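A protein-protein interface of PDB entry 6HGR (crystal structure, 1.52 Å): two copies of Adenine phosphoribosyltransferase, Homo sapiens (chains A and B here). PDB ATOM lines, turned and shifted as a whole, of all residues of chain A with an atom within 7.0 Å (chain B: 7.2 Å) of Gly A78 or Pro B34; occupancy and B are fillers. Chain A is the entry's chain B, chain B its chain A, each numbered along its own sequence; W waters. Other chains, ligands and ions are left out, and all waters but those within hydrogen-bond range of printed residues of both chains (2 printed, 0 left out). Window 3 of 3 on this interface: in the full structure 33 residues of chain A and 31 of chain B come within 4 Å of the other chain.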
ATOM      1  N   ASP A  57     -20.106   4.801 -20.110  1.00  0.00           N
ATOM      2  CA  ASP A  57     -20.800   3.771 -19.345  1.00  0.00           C
ATOM      3  C   ASP A  57     -20.319   2.361 -19.692  1.00  0.00           C
ATOM      4  O   ASP A  57     -20.158   1.533 -18.810  1.00  0.00           O
ATOM      5  CB  ASP A  57     -22.316   3.873 -19.533  1.00  0.00           C
ATOM      6  CG  ASP A  57     -22.897   5.160 -18.952  1.00  0.00           C
ATOM      7  OD1 ASP A  57     -22.568   5.480 -17.799  1.00  0.00           O
ATOM      8  OD2 ASP A  57     -23.688   5.840 -19.644  1.00  0.00           O
ATOM      9  N   TYR A  58     -20.140   2.095 -20.982  1.00  0.00           N
ATOM     10  CA  TYR A  58     -19.812   0.759 -21.482  1.00  0.00           C
ATOM     11  C   TYR A  58     -18.918   0.857 -22.706  1.00  0.00           C
ATOM     12  O   TYR A  58     -18.980   1.820 -23.494  1.00  0.00           O
ATOM     13  CB  TYR A  58     -21.073  -0.037 -21.874  1.00  0.00           C
ATOM     14  CG  TYR A  58     -21.952  -0.406 -20.705  1.00  0.00           C
ATOM     15  CD1 TYR A  58     -21.615  -1.447 -19.863  1.00  0.00           C
ATOM     16  CD2 TYR A  58     -23.113   0.313 -20.433  1.00  0.00           C
ATOM     17  CE1 TYR A  58     -22.390  -1.767 -18.775  1.00  0.00           C
ATOM     18  CE2 TYR A  58     -23.909  -0.014 -19.349  1.00  0.00           C
ATOM     19  CZ  TYR A  58     -23.534  -1.057 -18.522  1.00  0.00           C
ATOM     20  OH  TYR A  58     -24.304  -1.414 -17.431  1.00  0.00           O
ATOM     21  N   SER A  72     -10.675  -6.276 -22.300  1.00  0.00           N
ATOM     22  CA  SER A  72      -9.498  -5.757 -21.631  1.00  0.00           C
ATOM     23  C   SER A  72      -9.550  -4.248 -21.515  1.00  0.00           C
ATOM     24  O   SER A  72      -9.139  -3.676 -20.512  1.00  0.00           O
ATOM     25  CB  SER A  72      -8.213  -6.173 -22.354  1.00  0.00           C
ATOM     26  OG  SER A  72      -8.007  -7.570 -22.239  1.00  0.00           O
ATOM     27  N   LEU A  73     -10.068  -3.591 -22.547  1.00  0.00           N
ATOM     28  CA  LEU A  73     -10.195  -2.135 -22.498  1.00  0.00           C
ATOM     29  C   LEU A  73     -11.221  -1.719 -21.471  1.00  0.00           C
ATOM     30  O   LEU A  73     -10.986  -0.822 -20.661  1.00  0.00           O
ATOM     31  CB  LEU A  73     -10.530  -1.582 -23.886  1.00  0.00           C
ATOM     32  CG  LEU A  73     -10.768  -0.085 -23.998  1.00  0.00           C
ATOM     33  CD1 LEU A  73      -9.536   0.667 -23.526  1.00  0.00           C
ATOM     34  CD2 LEU A  73     -11.095   0.305 -25.425  1.00  0.00           C
ATOM     35  N   ALA A  74     -12.370  -2.377 -21.500  1.00  0.00           N
ATOM     36  CA  ALA A  74     -13.387  -2.183 -20.479  1.00  0.00           C
ATOM     37  C   ALA A  74     -12.823  -2.361 -19.055  1.00  0.00           C
ATOM     38  O   ALA A  74     -13.029  -1.516 -18.183  1.00  0.00           O
ATOM     39  CB  ALA A  74     -14.569  -3.109 -20.741  1.00  0.00           C
ATOM     40  N   GLN A  75     -12.113  -3.454 -18.835  1.00  0.00           N
ATOM     41  CA  GLN A  75     -11.530  -3.727 -17.520  1.00  0.00           C
ATOM     42  C   GLN A  75     -10.558  -2.622 -17.095  1.00  0.00           C
ATOM     43  O   GLN A  75     -10.576  -2.173 -15.944  1.00  0.00           O
ATOM     44  CB  GLN A  75     -10.841  -5.081 -17.527  1.00  0.00           C
ATOM     45  CG  GLN A  75     -11.774  -6.260 -17.388  1.00  0.00           C
ATOM     46  CD  GLN A  75     -12.261  -6.444 -15.964  1.00  0.00           C
ATOM     47  OE1 GLN A  75     -11.471  -6.710 -15.064  1.00  0.00           O
ATOM     48  NE2 GLN A  75     -13.558  -6.305 -15.753  1.00  0.00           N
ATOM     49  N   GLU A  76      -9.721  -2.161 -18.029  1.00  0.00           N
ATOM     50  CA  GLU A  76      -8.775  -1.091 -17.730  1.00  0.00           C
ATOM     51  C   GLU A  76      -9.479   0.191 -17.291  1.00  0.00           C
ATOM     52  O   GLU A  76      -8.977   0.953 -16.452  1.00  0.00           O
ATOM     53  CB  GLU A  76      -7.864  -0.850 -18.932  1.00  0.00           C
ATOM     54  CG  GLU A  76      -6.831   0.245 -18.737  1.00  0.00           C
ATOM     55  CD  GLU A  76      -5.798  -0.065 -17.664  1.00  0.00           C
ATOM     56  OE1 GLU A  76      -5.666  -1.242 -17.270  1.00  0.00           O
ATOM     57  OE2 GLU A  76      -5.117   0.882 -17.213  1.00  0.00           O
ATOM     58  N   LEU A  77     -10.674   0.405 -17.828  1.00  0.00           N
ATOM     59  CA  LEU A  77     -11.482   1.562 -17.523  1.00  0.00           C
ATOM     60  C   LEU A  77     -12.483   1.356 -16.371  1.00  0.00           C
ATOM     61  O   LEU A  77     -13.203   2.276 -16.000  1.00  0.00           O
ATOM     62  CB  LEU A  77     -12.233   1.981 -18.794  1.00  0.00           C
ATOM     63  CG  LEU A  77     -11.382   2.552 -19.939  1.00  0.00           C
ATOM     64  CD1 LEU A  77     -12.205   2.684 -21.216  1.00  0.00           C
ATOM     65  CD2 LEU A  77     -10.783   3.902 -19.559  1.00  0.00           C
ATOM     66  N   GLY A  78     -12.563   0.137 -15.849  1.00  0.00           N
ATOM     67  CA  GLY A  78     -13.491  -0.185 -14.773  1.00  0.00           C
ATOM     68  C   GLY A  78     -14.934  -0.328 -15.246  1.00  0.00           C
ATOM     69  O   GLY A  78     -15.868  -0.087 -14.479  1.00  0.00           O
ATOM     70  N   LEU A  79     -15.107  -0.692 -16.511  1.00  0.00           N
ATOM     71  CA  LEU A  79     -16.426  -0.724 -17.152  1.00  0.00           C
ATOM     72  C   LEU A  79     -16.770  -2.130 -17.604  1.00  0.00           C
ATOM     73  O   LEU A  79     -15.883  -2.982 -17.757  1.00  0.00           O
ATOM     74  CB  LEU A  79     -16.432   0.178 -18.381  1.00  0.00           C
ATOM     75  CG  LEU A  79     -16.067   1.643 -18.150  1.00  0.00           C
ATOM     76  CD1 LEU A  79     -16.081   2.373 -19.481  1.00  0.00           C
ATOM     77  CD2 LEU A  79     -17.014   2.285 -17.156  1.00  0.00           C
ATOM     78  N   GLY A  80     -18.057  -2.352 -17.840  1.00  0.00           N
ATOM     79  CA  GLY A  80     -18.487  -3.537 -18.553  1.00  0.00           C
ATOM     80  C   GLY A  80     -18.374  -3.379 -20.059  1.00  0.00           C
ATOM     81  O   GLY A  80     -18.113  -2.289 -20.597  1.00  0.00           O
ATOM     82  N   CYS A  81     -18.496  -4.511 -20.742  1.00  0.00           N
ATOM     83  CA  CYS A  81     -18.412  -4.574 -22.183  1.00  0.00           C
ATOM     84  C   CYS A  81     -19.697  -5.219 -22.701  1.00  0.00           C
ATOM     85  O   CYS A  81     -20.140  -6.235 -22.162  1.00  0.00           O
ATOM     86  CB  CYS A  81     -17.197  -5.407 -22.565  1.00  0.00           C
ATOM     87  SG  CYS A  81     -16.845  -5.501 -24.315  1.00  0.00           S
ATOM     88  N   PRO B  29     -23.966 -11.369 -19.803  1.00  0.00           N
ATOM     89  CA  PRO B  29     -24.003 -10.518 -18.606  1.00  0.00           C
ATOM     90  C   PRO B  29     -22.717 -10.567 -17.767  1.00  0.00           C
ATOM     91  O   PRO B  29     -22.446  -9.639 -17.004  1.00  0.00           O
ATOM     92  CB  PRO B  29     -25.178 -11.068 -17.808  1.00  0.00           C
ATOM     93  CG  PRO B  29     -26.010 -11.789 -18.802  1.00  0.00           C
ATOM     94  CD  PRO B  29     -25.045 -12.376 -19.787  1.00  0.00           C
ATOM     95  N   VAL B  30     -21.948 -11.634 -17.903  1.00  0.00           N
ATOM     96  CA  VAL B  30     -20.635 -11.724 -17.254  1.00  0.00           C
ATOM     97  C   VAL B  30     -19.722 -10.621 -17.784  1.00  0.00           C
ATOM     98  O   VAL B  30     -19.010  -9.962 -17.027  1.00  0.00           O
ATOM     99  CB  VAL B  30     -19.942 -13.089 -17.491  1.00  0.00           C
ATOM    100  CG1 VAL B  30     -18.537 -13.061 -16.931  1.00  0.00           C
ATOM    101  CG2 VAL B  30     -20.734 -14.230 -16.891  1.00  0.00           C
ATOM    102  N   LEU B  31     -19.757 -10.399 -19.094  1.00  0.00           N
ATOM    103  CA  LEU B  31     -18.939  -9.339 -19.694  1.00  0.00           C
ATOM    104  C   LEU B  31     -19.414  -7.947 -19.295  1.00  0.00           C
ATOM    105  O   LEU B  31     -18.618  -7.009 -19.207  1.00  0.00           O
ATOM    106  CB  LEU B  31     -18.955  -9.438 -21.218  1.00  0.00           C
ATOM    107  CG  LEU B  31     -17.967 -10.401 -21.878  1.00  0.00           C
ATOM    108  CD1 LEU B  31     -16.524  -9.958 -21.700  1.00  0.00           C
ATOM    109  CD2 LEU B  31     -18.174 -11.800 -21.370  1.00  0.00           C
ATOM    110  N   LYS B  32     -20.725  -7.793 -19.136  1.00  0.00           N
ATOM    111  CA  LYS B  32     -21.314  -6.487 -18.865  1.00  0.00           C
ATOM    112  C   LYS B  32     -21.069  -6.017 -17.435  1.00  0.00           C
ATOM    113  O   LYS B  32     -21.066  -4.831 -17.166  1.00  0.00           O
ATOM    114  CB  LYS B  32     -22.810  -6.510 -19.175  1.00  0.00           C
ATOM    115  CG  LYS B  32     -23.466  -5.138 -19.123  1.00  0.00           C
ATOM    116  CD  LYS B  32     -24.873  -5.190 -19.669  1.00  0.00           C
ATOM    117  CE  LYS B  32     -25.497  -3.811 -19.610  1.00  0.00           C
ATOM    118  NZ  LYS B  32     -26.949  -3.882 -19.874  1.00  0.00           N
ATOM    119  N   ASP B  33     -20.822  -6.961 -16.523  1.00  0.00           N
ATOM    120  CA  ASP B  33     -20.570  -6.632 -15.133  1.00  0.00           C
ATOM    121  C   ASP B  33     -19.068  -6.765 -14.872  1.00  0.00           C
ATOM    122  O   ASP B  33     -18.540  -7.877 -14.865  1.00  0.00           O
ATOM    123  CB  ASP B  33     -21.341  -7.605 -14.248  1.00  0.00           C
ATOM    124  CG  ASP B  33     -21.124  -7.363 -12.769  1.00  0.00           C
ATOM    125  OD1 ASP B  33     -20.194  -6.614 -12.382  1.00  0.00           O
ATOM    126  OD2 ASP B  33     -21.873  -7.976 -11.987  1.00  0.00           O
ATOM    127  N   PRO B  34     -18.358  -5.648 -14.692  1.00  0.00           N
ATOM    128  CA  PRO B  34     -16.901  -5.784 -14.631  1.00  0.00           C
ATOM    129  C   PRO B  34     -16.417  -6.639 -13.478  1.00  0.00           C
ATOM    130  O   PRO B  34     -15.382  -7.278 -13.597  1.00  0.00           O
ATOM    131  CB  PRO B  34     -16.402  -4.352 -14.481  1.00  0.00           C
ATOM    132  CG  PRO B  34     -17.596  -3.553 -14.063  1.00  0.00           C
ATOM    133  CD  PRO B  34     -18.780  -4.238 -14.653  1.00  0.00           C
ATOM    134  N   ALA B  35     -17.146  -6.643 -12.367  1.00  0.00           N
ATOM    135  CA  ALA B  35     -16.782  -7.511 -11.250  1.00  0.00           C
ATOM    136  C   ALA B  35     -16.906  -8.993 -11.603  1.00  0.00           C
ATOM    137  O   ALA B  35     -16.104  -9.803 -11.139  1.00  0.00           O
ATOM    138  CB  ALA B  35     -17.652  -7.191 -10.038  1.00  0.00           C
ATOM    139  N   SER B  36     -17.916  -9.344 -12.382  1.00  0.00           N
ATOM    140  CA  SER B  36     -18.159 -10.715 -12.772  1.00  0.00           C
ATOM    141  C   SER B  36     -17.076 -11.178 -13.739  1.00  0.00           C
ATOM    142  O   SER B  36     -16.515 -12.263 -13.595  1.00  0.00           O
ATOM    143  CB  SER B  36     -19.541 -10.823 -13.417  1.00  0.00           C
ATOM    144  OG  SER B  36     -19.918 -12.174 -13.684  1.00  0.00           O
ATOM    145  N   PHE B  37     -16.743 -10.326 -14.709  1.00  0.00           N
ATOM    146  CA  PHE B  37     -15.712 -10.679 -15.668  1.00  0.00           C
ATOM    147  C   PHE B  37     -14.370 -10.883 -14.955  1.00  0.00           C
ATOM    148  O   PHE B  37     -13.664 -11.846 -15.209  1.00  0.00           O
ATOM    149  CB  PHE B  37     -15.596  -9.594 -16.740  1.00  0.00           C
ATOM    150  CG  PHE B  37     -14.583  -9.897 -17.797  1.00  0.00           C
ATOM    151  CD1 PHE B  37     -14.834 -10.821 -18.772  1.00  0.00           C
ATOM    152  CD2 PHE B  37     -13.336  -9.297 -17.755  1.00  0.00           C
ATOM    153  CE1 PHE B  37     -13.886 -11.101 -19.741  1.00  0.00           C
ATOM    154  CE2 PHE B  37     -12.378  -9.585 -18.714  1.00  0.00           C
ATOM    155  CZ  PHE B  37     -12.656 -10.495 -19.699  1.00  0.00           C
ATOM    156  N   ARG B  38     -14.029  -9.985 -14.048  1.00  0.00           N
ATOM    157  CA  ARG B  38     -12.778 -10.077 -13.312  1.00  0.00           C
ATOM    158  C   ARG B  38     -12.723 -11.352 -12.469  1.00  0.00           C
ATOM    159  O   ARG B  38     -11.673 -12.010 -12.369  1.00  0.00           O
ATOM    160  CB  ARG B  38     -12.613  -8.843 -12.419  1.00  0.00           C
ATOM    161  CG  ARG B  38     -11.344  -8.858 -11.573  1.00  0.00           C
ATOM    162  CD  ARG B  38     -11.044  -7.482 -10.990  1.00  0.00           C
ATOM    163  NE  ARG B  38     -12.248  -6.840 -10.467  1.00  0.00           N
ATOM    164  CZ  ARG B  38     -12.843  -5.786 -11.023  1.00  0.00           C
ATOM    165  NH1 ARG B  38     -13.936  -5.272 -10.471  1.00  0.00           N
ATOM    166  NH2 ARG B  38     -12.344  -5.242 -12.126  1.00  0.00           N
ATOM    167  N   ALA B  39     -13.858 -11.712 -11.882  1.00  0.00           N
ATOM    168  CA  ALA B  39     -13.936 -12.944 -11.091  1.00  0.00           C
ATOM    169  C   ALA B  39     -13.677 -14.172 -11.963  1.00  0.00           C
ATOM    170  O   ALA B  39     -12.920 -15.065 -11.591  1.00  0.00           O
ATOM    171  CB  ALA B  39     -15.286 -13.058 -10.406  1.00  0.00           C
ATOM    172  N   ALA B  40     -14.307 -14.214 -13.131  1.00  0.00           N
ATOM    173  CA  ALA B  40     -14.151 -15.338 -14.048  1.00  0.00           C
ATOM    174  C   ALA B  40     -12.686 -15.508 -14.456  1.00  0.00           C
ATOM    175  O   ALA B  40     -12.145 -16.603 -14.404  1.00  0.00           O
ATOM    176  CB  ALA B  40     -15.029 -15.133 -15.271  1.00  0.00           C
HETATM  177  O   HOH W   1     -11.978  -2.992 -13.501  1.00  0.00           O
HETATM  178  O   HOH W   2     -21.829  -2.692 -15.557  1.00  0.00           O
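NE2 of Gln A75 sits at hydrogen-bond distance from O of Pro B34 (3.0 Å). The backbone carbonyl oxygen (O) of Leu B31 is in hydrogen-bond range of the backbone NH (N) of Cys A81 (2.9 Å). NH2 of Arg B38 is in hydrogen-bond range of OE1 of Gln A75 (3.4 Å). The backbone NH (N) of Lys B32 sits at hydrogen-bond distance from the backbone carbonyl oxygen (O) of Cys A81 (3.5 Å).
Among the printed residues, merely in contact across the chains: Tyr A58 with Lys B32 (3.5 Å), Gln A75 with Phe B37 (3.4 Å), Gly A78 with Pro B34 (3.9 Å), Leu A79 with Pro B34 (3.6 Å), Gly A80 with Leu B31 (3.5 Å), Gly A80 with Lys B32 (3.2 Å) and Gly A80 with Pro B34 (3.8 Å).
O of Ala A74 lies within hydrogen-bond range of N of Leu A79, at 2.8 Å. The backbone NH (N) of Phe B37 is in hydrogen-bond range of the backbone carbonyl oxygen (O) of Val B30.
No position is printed for both chains. Of the 11 pairs that touch across the chains among the printed residues, none has its exchanged pair printed and touching as well.
Water W1 bridges NH2 of Arg B38 (2.7 Å) and O of Gln A75 (2.9 Å). Water W2 lies within hydrogen-bond range of O of Lys B32 and OH of Tyr A58.
Of the 12 printed residues of chain A, 6 touch a printed residue of chain B. Printed residues of chain A that touch a printed residue of chain B: Tyr A58, Gln A75, Gly A78, Leu A79, Gly A80 and Cys A81. Hydrophobic or aromatic side chains of chain A within 4 Å of the printed part of chain B: Tyr A58. Of the 12 printed residues of chain B, 5 touch a printed residue of chain A. Hydrophobic or aromatic side chains of chain B within 4 Å of the printed part of chain A: Leu B31, Pro B34 and Phe B37. Along chain B the printed residues that touch a printed residue of chain A span positions 31 to 38. Among the printed residues, no Asp or Glu carboxylate lies within 4 Å of a Lys or Arg side-chain nitrogen of the other chain.
Of the printed residues of chain B, Tyr A58 touches Lys B32. Leu A73 touches none of the printed residues of chain B. Of the printed residues of chain B, Gln A75 touches Pro B34 (3.0 Å), Phe B37 (3.4 Å) and Arg B38 (3.4 Å). Of chain B, only Pro B34 comes within 4 Å of Gly A78. Printed residues of chain A within 4 Å of Lys B32: Tyr A58 (3.5 Å), Gly A80 (3.2 Å) and Cys A81 (3.5 Å). Asp B33 touches none of the printed residues of chain A. Printed residues of chain A within 4 Å of Pro B34: Gln A75, Gly A78, Leu A79 and Gly A80. Of the printed residues of chain A, Phe B37 touches Gln A75 (3.4 Å). The nearest printed residue of chain B that does not touch Tyr A58 is Asp B33 (5.9 Å).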
